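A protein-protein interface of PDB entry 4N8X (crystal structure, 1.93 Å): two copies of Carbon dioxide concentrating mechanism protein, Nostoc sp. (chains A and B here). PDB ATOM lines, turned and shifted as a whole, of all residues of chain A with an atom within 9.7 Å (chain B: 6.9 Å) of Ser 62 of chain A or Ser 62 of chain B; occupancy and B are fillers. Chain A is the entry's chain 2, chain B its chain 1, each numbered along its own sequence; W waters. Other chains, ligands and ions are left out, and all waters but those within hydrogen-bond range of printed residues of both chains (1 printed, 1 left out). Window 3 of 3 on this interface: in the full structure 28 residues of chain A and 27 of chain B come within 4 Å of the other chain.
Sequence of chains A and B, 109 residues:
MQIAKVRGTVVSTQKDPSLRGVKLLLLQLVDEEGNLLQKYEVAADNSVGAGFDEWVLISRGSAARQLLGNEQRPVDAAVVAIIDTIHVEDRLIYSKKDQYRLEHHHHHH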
ATOM      1  N   SER A  59      24.052  10.123   8.877  1.00  0.00           N
ATOM      2  CA  SER A  59      23.281   8.927   9.183  1.00  0.00           C
ATOM      3  C   SER A  59      24.186   7.765   8.866  1.00  0.00           C
ATOM      4  O   SER A  59      24.910   7.811   7.861  1.00  0.00           O
ATOM      5  CB  SER A  59      22.062   8.817   8.298  1.00  0.00           C
ATOM      6  OG  SER A  59      21.262   9.963   8.369  1.00  0.00           O
ATOM      7  N   ARG A  60      24.086   6.714   9.679  1.00  0.00           N
ATOM      8  CA  ARG A  60      25.005   5.573   9.641  1.00  0.00           C
ATOM      9  C   ARG A  60      24.241   4.266   9.343  1.00  0.00           C
ATOM     10  O   ARG A  60      23.003   4.223   9.467  1.00  0.00           O
ATOM     11  CB  ARG A  60      25.736   5.428  11.002  1.00  0.00           C
ATOM     12  CG  ARG A  60      26.736   6.559  11.337  1.00  0.00           C
ATOM     13  CD  ARG A  60      27.464   6.332  12.701  1.00  0.00           C
ATOM     14  NE  ARG A  60      26.602   6.657  13.828  1.00  0.00           N
ATOM     15  CZ  ARG A  60      26.967   6.573  15.108  1.00  0.00           C
ATOM     16  NH1 ARG A  60      28.186   6.179  15.440  1.00  0.00           N
ATOM     17  NH2 ARG A  60      26.102   6.885  16.058  1.00  0.00           N
ATOM     18  N   GLY A  61      24.969   3.199   8.994  1.00  0.00           N
ATOM     19  CA  GLY A  61      24.298   1.936   8.701  1.00  0.00           C
ATOM     20  C   GLY A  61      23.501   2.059   7.405  1.00  0.00           C
ATOM     21  O   GLY A  61      23.816   2.899   6.547  1.00  0.00           O
ATOM     22  N   SER A  62      22.459   1.245   7.241  1.00  0.00           N
ATOM     23  CA  SER A  62      21.791   1.150   5.944  1.00  0.00           C
ATOM     24  C   SER A  62      21.039   2.423   5.632  1.00  0.00           C
ATOM     25  O   SER A  62      20.663   2.643   4.468  1.00  0.00           O
ATOM     26  CB  SER A  62      20.846  -0.051   5.905  1.00  0.00           C
ATOM     27  OG  SER A  62      19.835   0.108   6.889  1.00  0.00           O
ATOM     28  N   ALA A  63      20.813   3.273   6.653  1.00  0.00           N
ATOM     29  CA  ALA A  63      20.211   4.592   6.384  1.00  0.00           C
ATOM     30  C   ALA A  63      21.018   5.378   5.315  1.00  0.00           C
ATOM     31  O   ALA A  63      20.454   6.145   4.539  1.00  0.00           O
ATOM     32  CB  ALA A  63      20.024   5.444   7.696  1.00  0.00           C
ATOM     33  N   ALA A  64      22.332   5.157   5.289  1.00  0.00           N
ATOM     34  CA  ALA A  64      23.215   5.899   4.404  1.00  0.00           C
ATOM     35  C   ALA A  64      22.930   5.572   2.929  1.00  0.00           C
ATOM     36  O   ALA A  64      23.248   6.375   2.036  1.00  0.00           O
ATOM     37  CB  ALA A  64      24.684   5.642   4.774  1.00  0.00           C
ATOM     38  N   ARG A  65      22.297   4.421   2.682  1.00  0.00           N
ATOM     39  CA  ARG A  65      21.986   3.994   1.313  1.00  0.00           C
ATOM     40  C   ARG A  65      20.646   4.507   0.809  1.00  0.00           C
ATOM     41  O   ARG A  65      20.272   4.281  -0.345  1.00  0.00           O
ATOM     42  CB  ARG A  65      22.034   2.455   1.197  1.00  0.00           C
ATOM     43  CG  ARG A  65      23.393   1.852   1.559  1.00  0.00           C
ATOM     44  CD  ARG A  65      23.516   0.391   1.062  1.00  0.00           C
ATOM     45  NE  ARG A  65      22.274  -0.376   1.240  1.00  0.00           N
ATOM     46  CZ  ARG A  65      22.052  -1.252   2.220  1.00  0.00           C
ATOM     47  NH1 ARG A  65      22.984  -1.485   3.126  1.00  0.00           N
ATOM     48  NH2 ARG A  65      20.898  -1.898   2.299  1.00  0.00           N
ATOM     49  N   GLN A  66      19.900   5.169   1.680  1.00  0.00           N
ATOM     50  CA  GLN A  66      18.601   5.709   1.289  1.00  0.00           C
ATOM     51  C   GLN A  66      18.683   6.995   0.449  1.00  0.00           C
ATOM     52  O   GLN A  66      17.690   7.411  -0.130  1.00  0.00           O
ATOM     53  CB  GLN A  66      17.728   5.919   2.536  1.00  0.00           C
ATOM     54  CG  GLN A  66      17.703   4.667   3.393  1.00  0.00           C
ATOM     55  CD  GLN A  66      17.420   3.435   2.540  1.00  0.00           C
ATOM     56  OE1 GLN A  66      16.418   3.382   1.841  1.00  0.00           O
ATOM     57  NE2 GLN A  66      18.310   2.465   2.571  1.00  0.00           N
ATOM     58  N   LEU A  67      19.845   7.639   0.386  1.00  0.00           N
ATOM     59  CA  LEU A  67      19.966   8.821  -0.492  1.00  0.00           C
ATOM     60  C   LEU A  67      19.963   8.339  -1.935  1.00  0.00           C
ATOM     61  O   LEU A  67      20.622   7.339  -2.243  1.00  0.00           O
ATOM     62  CB  LEU A  67      21.280   9.560  -0.204  1.00  0.00           C
ATOM     63  CG  LEU A  67      21.469   9.948   1.263  1.00  0.00           C
ATOM     64  CD1 LEU A  67      22.731  10.773   1.435  1.00  0.00           C
ATOM     65  CD2 LEU A  67      20.244  10.742   1.744  1.00  0.00           C
ATOM     66  N   ASN A  70      22.741   6.173  -3.716  1.00  0.00           N
ATOM     67  CA  ASN A  70      23.515   5.341  -2.799  1.00  0.00           C
ATOM     68  C   ASN A  70      22.918   3.949  -2.636  1.00  0.00           C
ATOM     69  O   ASN A  70      23.470   3.122  -1.916  1.00  0.00           O
ATOM     70  CB  ASN A  70      23.566   5.990  -1.413  1.00  0.00           C
ATOM     71  CG  ASN A  70      24.590   7.115  -1.308  1.00  0.00           C
ATOM     72  OD1 ASN A  70      25.280   7.432  -2.273  1.00  0.00           O
ATOM     73  ND2 ASN A  70      24.684   7.728  -0.126  1.00  0.00           N
ATOM     74  N   GLU A  71      21.775   3.693  -3.274  1.00  0.00           N
ATOM     75  CA  GLU A  71      20.995   2.489  -2.978  1.00  0.00           C
ATOM     76  C   GLU A  71      21.793   1.172  -2.977  1.00  0.00           C
ATOM     77  O   GLU A  71      21.626   0.360  -2.069  1.00  0.00           O
ATOM     78  CB  GLU A  71      19.727   2.409  -3.846  1.00  0.00           C
ATOM     79  CG  GLU A  71      18.713   3.513  -3.513  1.00  0.00           C
ATOM     80  CD  GLU A  71      18.960   4.818  -4.279  1.00  0.00           C
ATOM     81  OE1 GLU A  71      20.012   4.933  -4.962  1.00  0.00           O
ATOM     82  OE2 GLU A  71      18.087   5.714  -4.209  1.00  0.00           O
ATOM     83  N   GLN A  72      22.676   0.972  -3.954  1.00  0.00           N
ATOM     84  CA  GLN A  72      23.482  -0.251  -3.965  1.00  0.00           C
ATOM     85  C   GLN A  72      24.959   0.010  -3.760  1.00  0.00           C
ATOM     86  O   GLN A  72      25.777  -0.806  -4.203  1.00  0.00           O
ATOM     87  CB  GLN A  72      23.324  -1.056  -5.275  1.00  0.00           C
ATOM     88  CG  GLN A  72      21.914  -1.412  -5.709  1.00  0.00           C
ATOM     89  CD  GLN A  72      20.957  -1.736  -4.563  1.00  0.00           C
ATOM     90  OE1 GLN A  72      21.327  -2.379  -3.574  1.00  0.00           O
ATOM     91  NE2 GLN A  72      19.708  -1.305  -4.707  1.00  0.00           N
ATOM     92  N   ARG A  73      25.303   1.130  -3.099  1.00  0.00           N
ATOM     93  CA  ARG A  73      26.688   1.474  -2.810  1.00  0.00           C
ATOM     94  C   ARG A  73      27.036   0.970  -1.413  1.00  0.00           C
ATOM     95  O   ARG A  73      26.219   1.073  -0.493  1.00  0.00           O
ATOM     96  CB  ARG A  73      26.912   3.001  -2.871  1.00  0.00           C
ATOM     97  CG  ARG A  73      26.660   3.636  -4.273  1.00  0.00           C
ATOM     98  CD  ARG A  73      27.229   5.050  -4.347  1.00  0.00           C
ATOM     99  NE  ARG A  73      27.317   5.556  -5.719  1.00  0.00           N
ATOM    100  CZ  ARG A  73      26.711   6.659  -6.136  1.00  0.00           C
ATOM    101  NH1 ARG A  73      26.836   7.052  -7.398  1.00  0.00           N
ATOM    102  NH2 ARG A  73      25.986   7.368  -5.280  1.00  0.00           N
ATOM    103  N   PRO A  74      28.224   0.397  -1.261  1.00  0.00           N
ATOM    104  CA  PRO A  74      28.709  -0.132   0.016  1.00  0.00           C
ATOM    105  C   PRO A  74      29.082   1.025   0.948  1.00  0.00           C
ATOM    106  O   PRO A  74      30.252   1.145   1.307  1.00  0.00           O
ATOM    107  CB  PRO A  74      29.989  -0.872  -0.381  1.00  0.00           C
ATOM    108  CG  PRO A  74      30.466  -0.117  -1.702  1.00  0.00           C
ATOM    109  CD  PRO A  74      29.140   0.093  -2.381  1.00  0.00           C
ATOM    110  N   VAL A  75      28.121   1.866   1.333  1.00  0.00           N
ATOM    111  CA  VAL A  75      28.460   3.004   2.194  1.00  0.00           C
ATOM    112  C   VAL A  75      27.641   2.875   3.447  1.00  0.00           C
ATOM    113  O   VAL A  75      26.462   2.504   3.377  1.00  0.00           O
ATOM    114  CB  VAL A  75      28.187   4.378   1.537  1.00  0.00           C
ATOM    115  CG1 VAL A  75      29.200   4.658   0.412  1.00  0.00           C
ATOM    116  CG2 VAL A  75      26.765   4.465   1.012  1.00  0.00           C
ATOM    117  N   ASP A  76      28.262   3.182   4.587  1.00  0.00           N
ATOM    118  CA  ASP A  76      27.609   3.005   5.889  1.00  0.00           C
ATOM    119  C   ASP A  76      27.639   4.319   6.677  1.00  0.00           C
ATOM    120  O   ASP A  76      27.337   4.359   7.861  1.00  0.00           O
ATOM    121  CB  ASP A  76      28.295   1.902   6.689  1.00  0.00           C
ATOM    122  CG  ASP A  76      29.734   2.232   7.006  1.00  0.00           C
ATOM    123  OD1 ASP A  76      30.187   3.362   6.698  1.00  0.00           O
ATOM    124  OD2 ASP A  76      30.422   1.351   7.566  1.00  0.00           O
ATOM    125  N   ALA A  77      28.001   5.398   5.994  1.00  0.00           N
ATOM    126  CA  ALA A  77      27.915   6.739   6.569  1.00  0.00           C
ATOM    127  C   ALA A  77      27.730   7.733   5.429  1.00  0.00           C
ATOM    128  O   ALA A  77      28.383   7.606   4.390  1.00  0.00           O
ATOM    129  CB  ALA A  77      29.170   7.055   7.385  1.00  0.00           C
ATOM    130  N   ALA A  78      26.847   8.721   5.628  1.00  0.00           N
ATOM    131  CA  ALA A  78      26.608   9.746   4.639  1.00  0.00           C
ATOM    132  C   ALA A  78      26.213  11.070   5.269  1.00  0.00           C
ATOM    133  O   ALA A  78      25.527  11.105   6.307  1.00  0.00           O
ATOM    134  CB  ALA A  78      25.527   9.290   3.625  1.00  0.00           C
ATOM    135  N   VAL A  80      23.778  13.928   5.454  1.00  0.00           N
ATOM    136  CA  VAL A  80      22.388  14.070   5.016  1.00  0.00           C
ATOM    137  C   VAL A  80      21.858  15.502   5.178  1.00  0.00           C
ATOM    138  O   VAL A  80      20.772  15.846   4.693  1.00  0.00           O
ATOM    139  CB  VAL A  80      21.499  13.069   5.757  1.00  0.00           C
ATOM    140  CG1 VAL A  80      22.031  11.665   5.503  1.00  0.00           C
ATOM    141  CG2 VAL A  80      21.542  13.353   7.274  1.00  0.00           C
ATOM    142  N   ARG B  60      30.957  -1.343   7.134  1.00  0.00           N
ATOM    143  CA  ARG B  60      30.488  -2.415   8.049  1.00  0.00           C
ATOM    144  C   ARG B  60      28.981  -2.562   7.992  1.00  0.00           C
ATOM    145  O   ARG B  60      28.273  -1.638   7.543  1.00  0.00           O
ATOM    146  CB  ARG B  60      31.006  -2.190   9.512  1.00  0.00           C
ATOM    147  CG  ARG B  60      30.716  -3.356  10.583  1.00  0.00           C
ATOM    148  CD  ARG B  60      31.954  -4.230  11.089  1.00  0.00           C
ATOM    149  NE  ARG B  60      31.564  -5.460  11.823  1.00  0.00           N
ATOM    150  CZ  ARG B  60      32.385  -6.335  12.451  1.00  0.00           C
ATOM    151  NH1 ARG B  60      33.715  -6.182  12.495  1.00  0.00           N
ATOM    152  NH2 ARG B  60      31.853  -7.411  13.055  1.00  0.00           N
ATOM    153  N   GLY B  61      28.471  -3.721   8.414  1.00  0.00           N
ATOM    154  CA  GLY B  61      27.036  -3.962   8.406  1.00  0.00           C
ATOM    155  C   GLY B  61      26.586  -4.369   7.011  1.00  0.00           C
ATOM    156  O   GLY B  61      27.414  -4.807   6.210  1.00  0.00           O
ATOM    157  N   SER B  62      25.306  -4.184   6.703  1.00  0.00           N
ATOM    158  CA  SER B  62      24.733  -4.573   5.390  1.00  0.00           C
ATOM    159  C   SER B  62      25.418  -3.873   4.211  1.00  0.00           C
ATOM    160  O   SER B  62      25.385  -4.383   3.095  1.00  0.00           O
ATOM    161  CB  SER B  62      23.197  -4.377   5.333  1.00  0.00           C
ATOM    162  OG  SER B  62      22.825  -3.012   5.570  1.00  0.00           O
ATOM    163  N   ALA B  63      26.059  -2.727   4.453  1.00  0.00           N
ATOM    164  CA  ALA B  63      26.865  -2.078   3.411  1.00  0.00           C
ATOM    165  C   ALA B  63      27.850  -3.086   2.783  1.00  0.00           C
ATOM    166  O   ALA B  63      28.144  -3.023   1.607  1.00  0.00           O
ATOM    167  CB  ALA B  63      27.660  -0.898   4.001  1.00  0.00           C
ATOM    168  N   ALA B  64      28.382  -3.997   3.587  1.00  0.00           N
ATOM    169  CA  ALA B  64      29.438  -4.869   3.081  1.00  0.00           C
ATOM    170  C   ALA B  64      28.857  -5.843   2.100  1.00  0.00           C
ATOM    171  O   ALA B  64      29.591  -6.474   1.338  1.00  0.00           O
ATOM    172  CB  ALA B  64      30.152  -5.594   4.230  1.00  0.00           C
ATOM    173  N   ARG B  65      27.529  -5.976   2.103  1.00  0.00           N
ATOM    174  CA  ARG B  65      26.893  -6.956   1.223  1.00  0.00           C
ATOM    175  C   ARG B  65      26.491  -6.320  -0.105  1.00  0.00           C
ATOM    176  O   ARG B  65      25.981  -7.002  -0.992  1.00  0.00           O
ATOM    177  CB  ARG B  65      25.689  -7.678   1.908  1.00  0.00           C
ATOM    178  CG  ARG B  65      26.043  -8.383   3.268  1.00  0.00           C
ATOM    179  CD  ARG B  65      25.003  -9.393   3.777  1.00  0.00           C
ATOM    180  NE  ARG B  65      23.816  -8.767   4.404  1.00  0.00           N
ATOM    181  CZ  ARG B  65      22.642  -8.625   3.794  1.00  0.00           C
ATOM    182  NH1 ARG B  65      21.624  -8.050   4.415  1.00  0.00           N
ATOM    183  NH2 ARG B  65      22.489  -9.050   2.553  1.00  0.00           N
ATOM    184  N   GLN B  66      26.731  -5.022  -0.266  1.00  0.00           N
ATOM    185  CA  GLN B  66      26.394  -4.401  -1.567  1.00  0.00           C
ATOM    186  C   GLN B  66      27.459  -4.662  -2.633  1.00  0.00           C
ATOM    187  O   GLN B  66      27.212  -4.448  -3.806  1.00  0.00           O
ATOM    188  CB  GLN B  66      26.114  -2.896  -1.456  1.00  0.00           C
ATOM    189  CG  GLN B  66      25.233  -2.500  -0.293  1.00  0.00           C
ATOM    190  CD  GLN B  66      23.892  -3.168  -0.352  1.00  0.00           C
ATOM    191  OE1 GLN B  66      23.164  -3.040  -1.347  1.00  0.00           O
ATOM    192  NE2 GLN B  66      23.554  -3.921   0.706  1.00  0.00           N
ATOM    193  N   LEU B  67      28.640  -5.099  -2.235  1.00  0.00           N
ATOM    194  CA  LEU B  67      29.665  -5.464  -3.216  1.00  0.00           C
ATOM    195  C   LEU B  67      29.123  -6.649  -3.988  1.00  0.00           C
ATOM    196  O   LEU B  67      28.387  -7.460  -3.420  1.00  0.00           O
ATOM    197  CB  LEU B  67      30.979  -5.863  -2.529  1.00  0.00           C
ATOM    198  CG  LEU B  67      31.666  -4.889  -1.567  1.00  0.00           C
ATOM    199  CD1 LEU B  67      33.070  -5.381  -1.228  1.00  0.00           C
ATOM    200  CD2 LEU B  67      31.727  -3.520  -2.187  1.00  0.00           C
ATOM    201  N   VAL B  75      28.936 -11.471   5.539  1.00  0.00           N
ATOM    202  CA  VAL B  75      30.059 -10.587   5.741  1.00  0.00           C
ATOM    203  C   VAL B  75      29.489  -9.286   6.284  1.00  0.00           C
ATOM    204  O   VAL B  75      28.460  -8.789   5.808  1.00  0.00           O
ATOM    205  CB  VAL B  75      30.813 -10.357   4.438  1.00  0.00           C
ATOM    206  CG1 VAL B  75      31.322 -11.692   3.905  1.00  0.00           C
ATOM    207  CG2 VAL B  75      29.889  -9.759   3.414  1.00  0.00           C
ATOM    208  N   ASP B  76      30.133  -8.757   7.315  1.00  0.00           N
ATOM    209  CA  ASP B  76      29.631  -7.541   7.923  1.00  0.00           C
ATOM    210  C   ASP B  76      30.710  -6.497   7.888  1.00  0.00           C
ATOM    211  O   ASP B  76      30.582  -5.470   8.552  1.00  0.00           O
ATOM    212  CB  ASP B  76      29.196  -7.804   9.372  1.00  0.00           C
ATOM    213  CG  ASP B  76      30.313  -8.423  10.218  1.00  0.00           C
ATOM    214  OD1 ASP B  76      31.447  -8.555   9.700  1.00  0.00           O
ATOM    215  OD2 ASP B  76      30.046  -8.764  11.402  1.00  0.00           O
HETATM  216  O   HOH W   1      27.129  -2.527  -5.923  1.00  0.00           O
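NH1 of Arg 65 of chain A is in hydrogen-bond range of OG of Ser 62 of chain B, 2.9 Å away. OD2 of Asp 76 of chain A lies within hydrogen-bond range of N of Arg 60 of chain B. The guanidinium group (NH1) of Arg 65 of chain A lies close to the side-chain amide nitrogen (NE2) of Gln 66 of chain B (3.5 Å). OE1 of Gln 72 of chain A lies close to OE1 of Gln 66 of chain B.
Of chain B, only Ser 62 (3.6 Å) comes within 4 Å of Ser 62 of chain A. Ala 64 of chain A touches none of the printed residues of chain B. Printed residues of chain B within 4 Å of Arg 73 of chain A: Gln 66 (3.7 Å). Of the printed residues of chain B, Val 75 of chain A touches Ala 63 (3.7 Å). Ala 78 of chain A touches none of the printed residues of chain B. No residue of chain A comes within 4 Å of Gly 61 of chain B. Of the printed residues of chain A, Ser 62 of chain B touches Ser 62 and Arg 65. Of chain A, only Arg 65, Pro 74, Val 75 and Asp 76 come within 4 Å of Ala 63 of chain B. No residue of chain A comes within 4 Å of Ala 64 of chain B. Printed residues of chain A within 4 Å of Leu 67 of chain B: Pro 74 (3.6 Å). The nearest residue of chain B that does not touch Ser 62 of chain A is Ala 63 of chain B (6.0 Å). The nearest residue of chain A that does not touch Ser 62 of chain B is Gly 61 of chain A (5.4 Å). The nearest printed residue of chain A that does not touch Leu 67 of chain B is Gln 72 of chain A (5.5 Å).
Ser 62 of chain B touches its own counterpart, Ser 62 of chain A. Arg 65 of chain A touches Ser 62 of chain B, but with the chains exchanged Ser 62 of chain A does not touch Arg 65 of chain B (8.2 Å). Asp 76 of chain A touches Arg 60 of chain B, but with the chains exchanged Arg 60 of chain A does not touch Asp 76 of chain B (11.6 Å). Asp 76 of chain A touches Ala 63 of chain B, but with the chains exchanged Ala 63 of chain A does not touch Asp 76 of chain B (13.2 Å). Of the 13 pairs that touch across the chains among the printed residues, 1 has its exchanged pair printed and touching as well.
Of the 10 printed residues of chain B, 5 touch a printed residue of chain A. Printed residues of chain A that touch a printed residue of chain B: Ser 62, Arg 65, Glu 71, Gln 72, Arg 73, Pro 74, Val 75 and Asp 76. Among the printed residues, 13 pairs touch across the chains.
The backbone NH of Gly 61 of chain A lies within hydrogen-bond range of the backbone carbonyl oxygen of Asp 76 of chain A. The guanidinium group (NH2) of Arg 73 of chain A lies within hydrogen-bond range of the side-chain amide oxygen (OD1) of Asn 70 of chain A, at 3.1 Å. O of Ser 62 of chain A is in hydrogen-bond range of NE2 of Gln 66 of chain A (3.0 Å). The backbone NH (N) of Glu 71 of chain A lies close to the backbone carbonyl oxygen (O) of Arg 65 of chain A (3.3 Å). The side-chain amide nitrogen (NE2) of Gln 66 of chain B sits at hydrogen-bond distance from the backbone carbonyl oxygen (O) of Ser 62 of chain B, at 3.0 Å. NH2 of Arg 60 of chain B is in salt-bridge range of OD2 of Asp 76 of chain B (2.8 Å).
OG of Ser 62 of chain B touches CB of Ser 62 of chain A (3.6 Å). Arg 65 of chain A touches Ala 63 of chain B (NH1 to N, 3.6 Å). Gln 66 of chain B touches Glu 71 of chain A. CG of Gln 66 of chain B touches O of Arg 73 of chain A, at 3.7 Å. CA of Pro 74 of chain A touches O of Ala 63 of chain B (3.3 Å). Pro 74 of chain A touches Gln 66 of chain B (N to CB, 3.9 Å). Leu 67 of chain B touches Pro 74 of chain A. CB of Ala 63 of chain B touches O of Val 75 of chain A, at 3.7 Å. Ala 63 of chain B touches Asp 76 of chain A.
Water W1 lies within hydrogen-bond range of the backbone carbonyl oxygen (O) of Gln 72 of chain A (2.8 Å) and the backbone carbonyl oxygen (O) of Gln 66 of chain B (2.9 Å).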
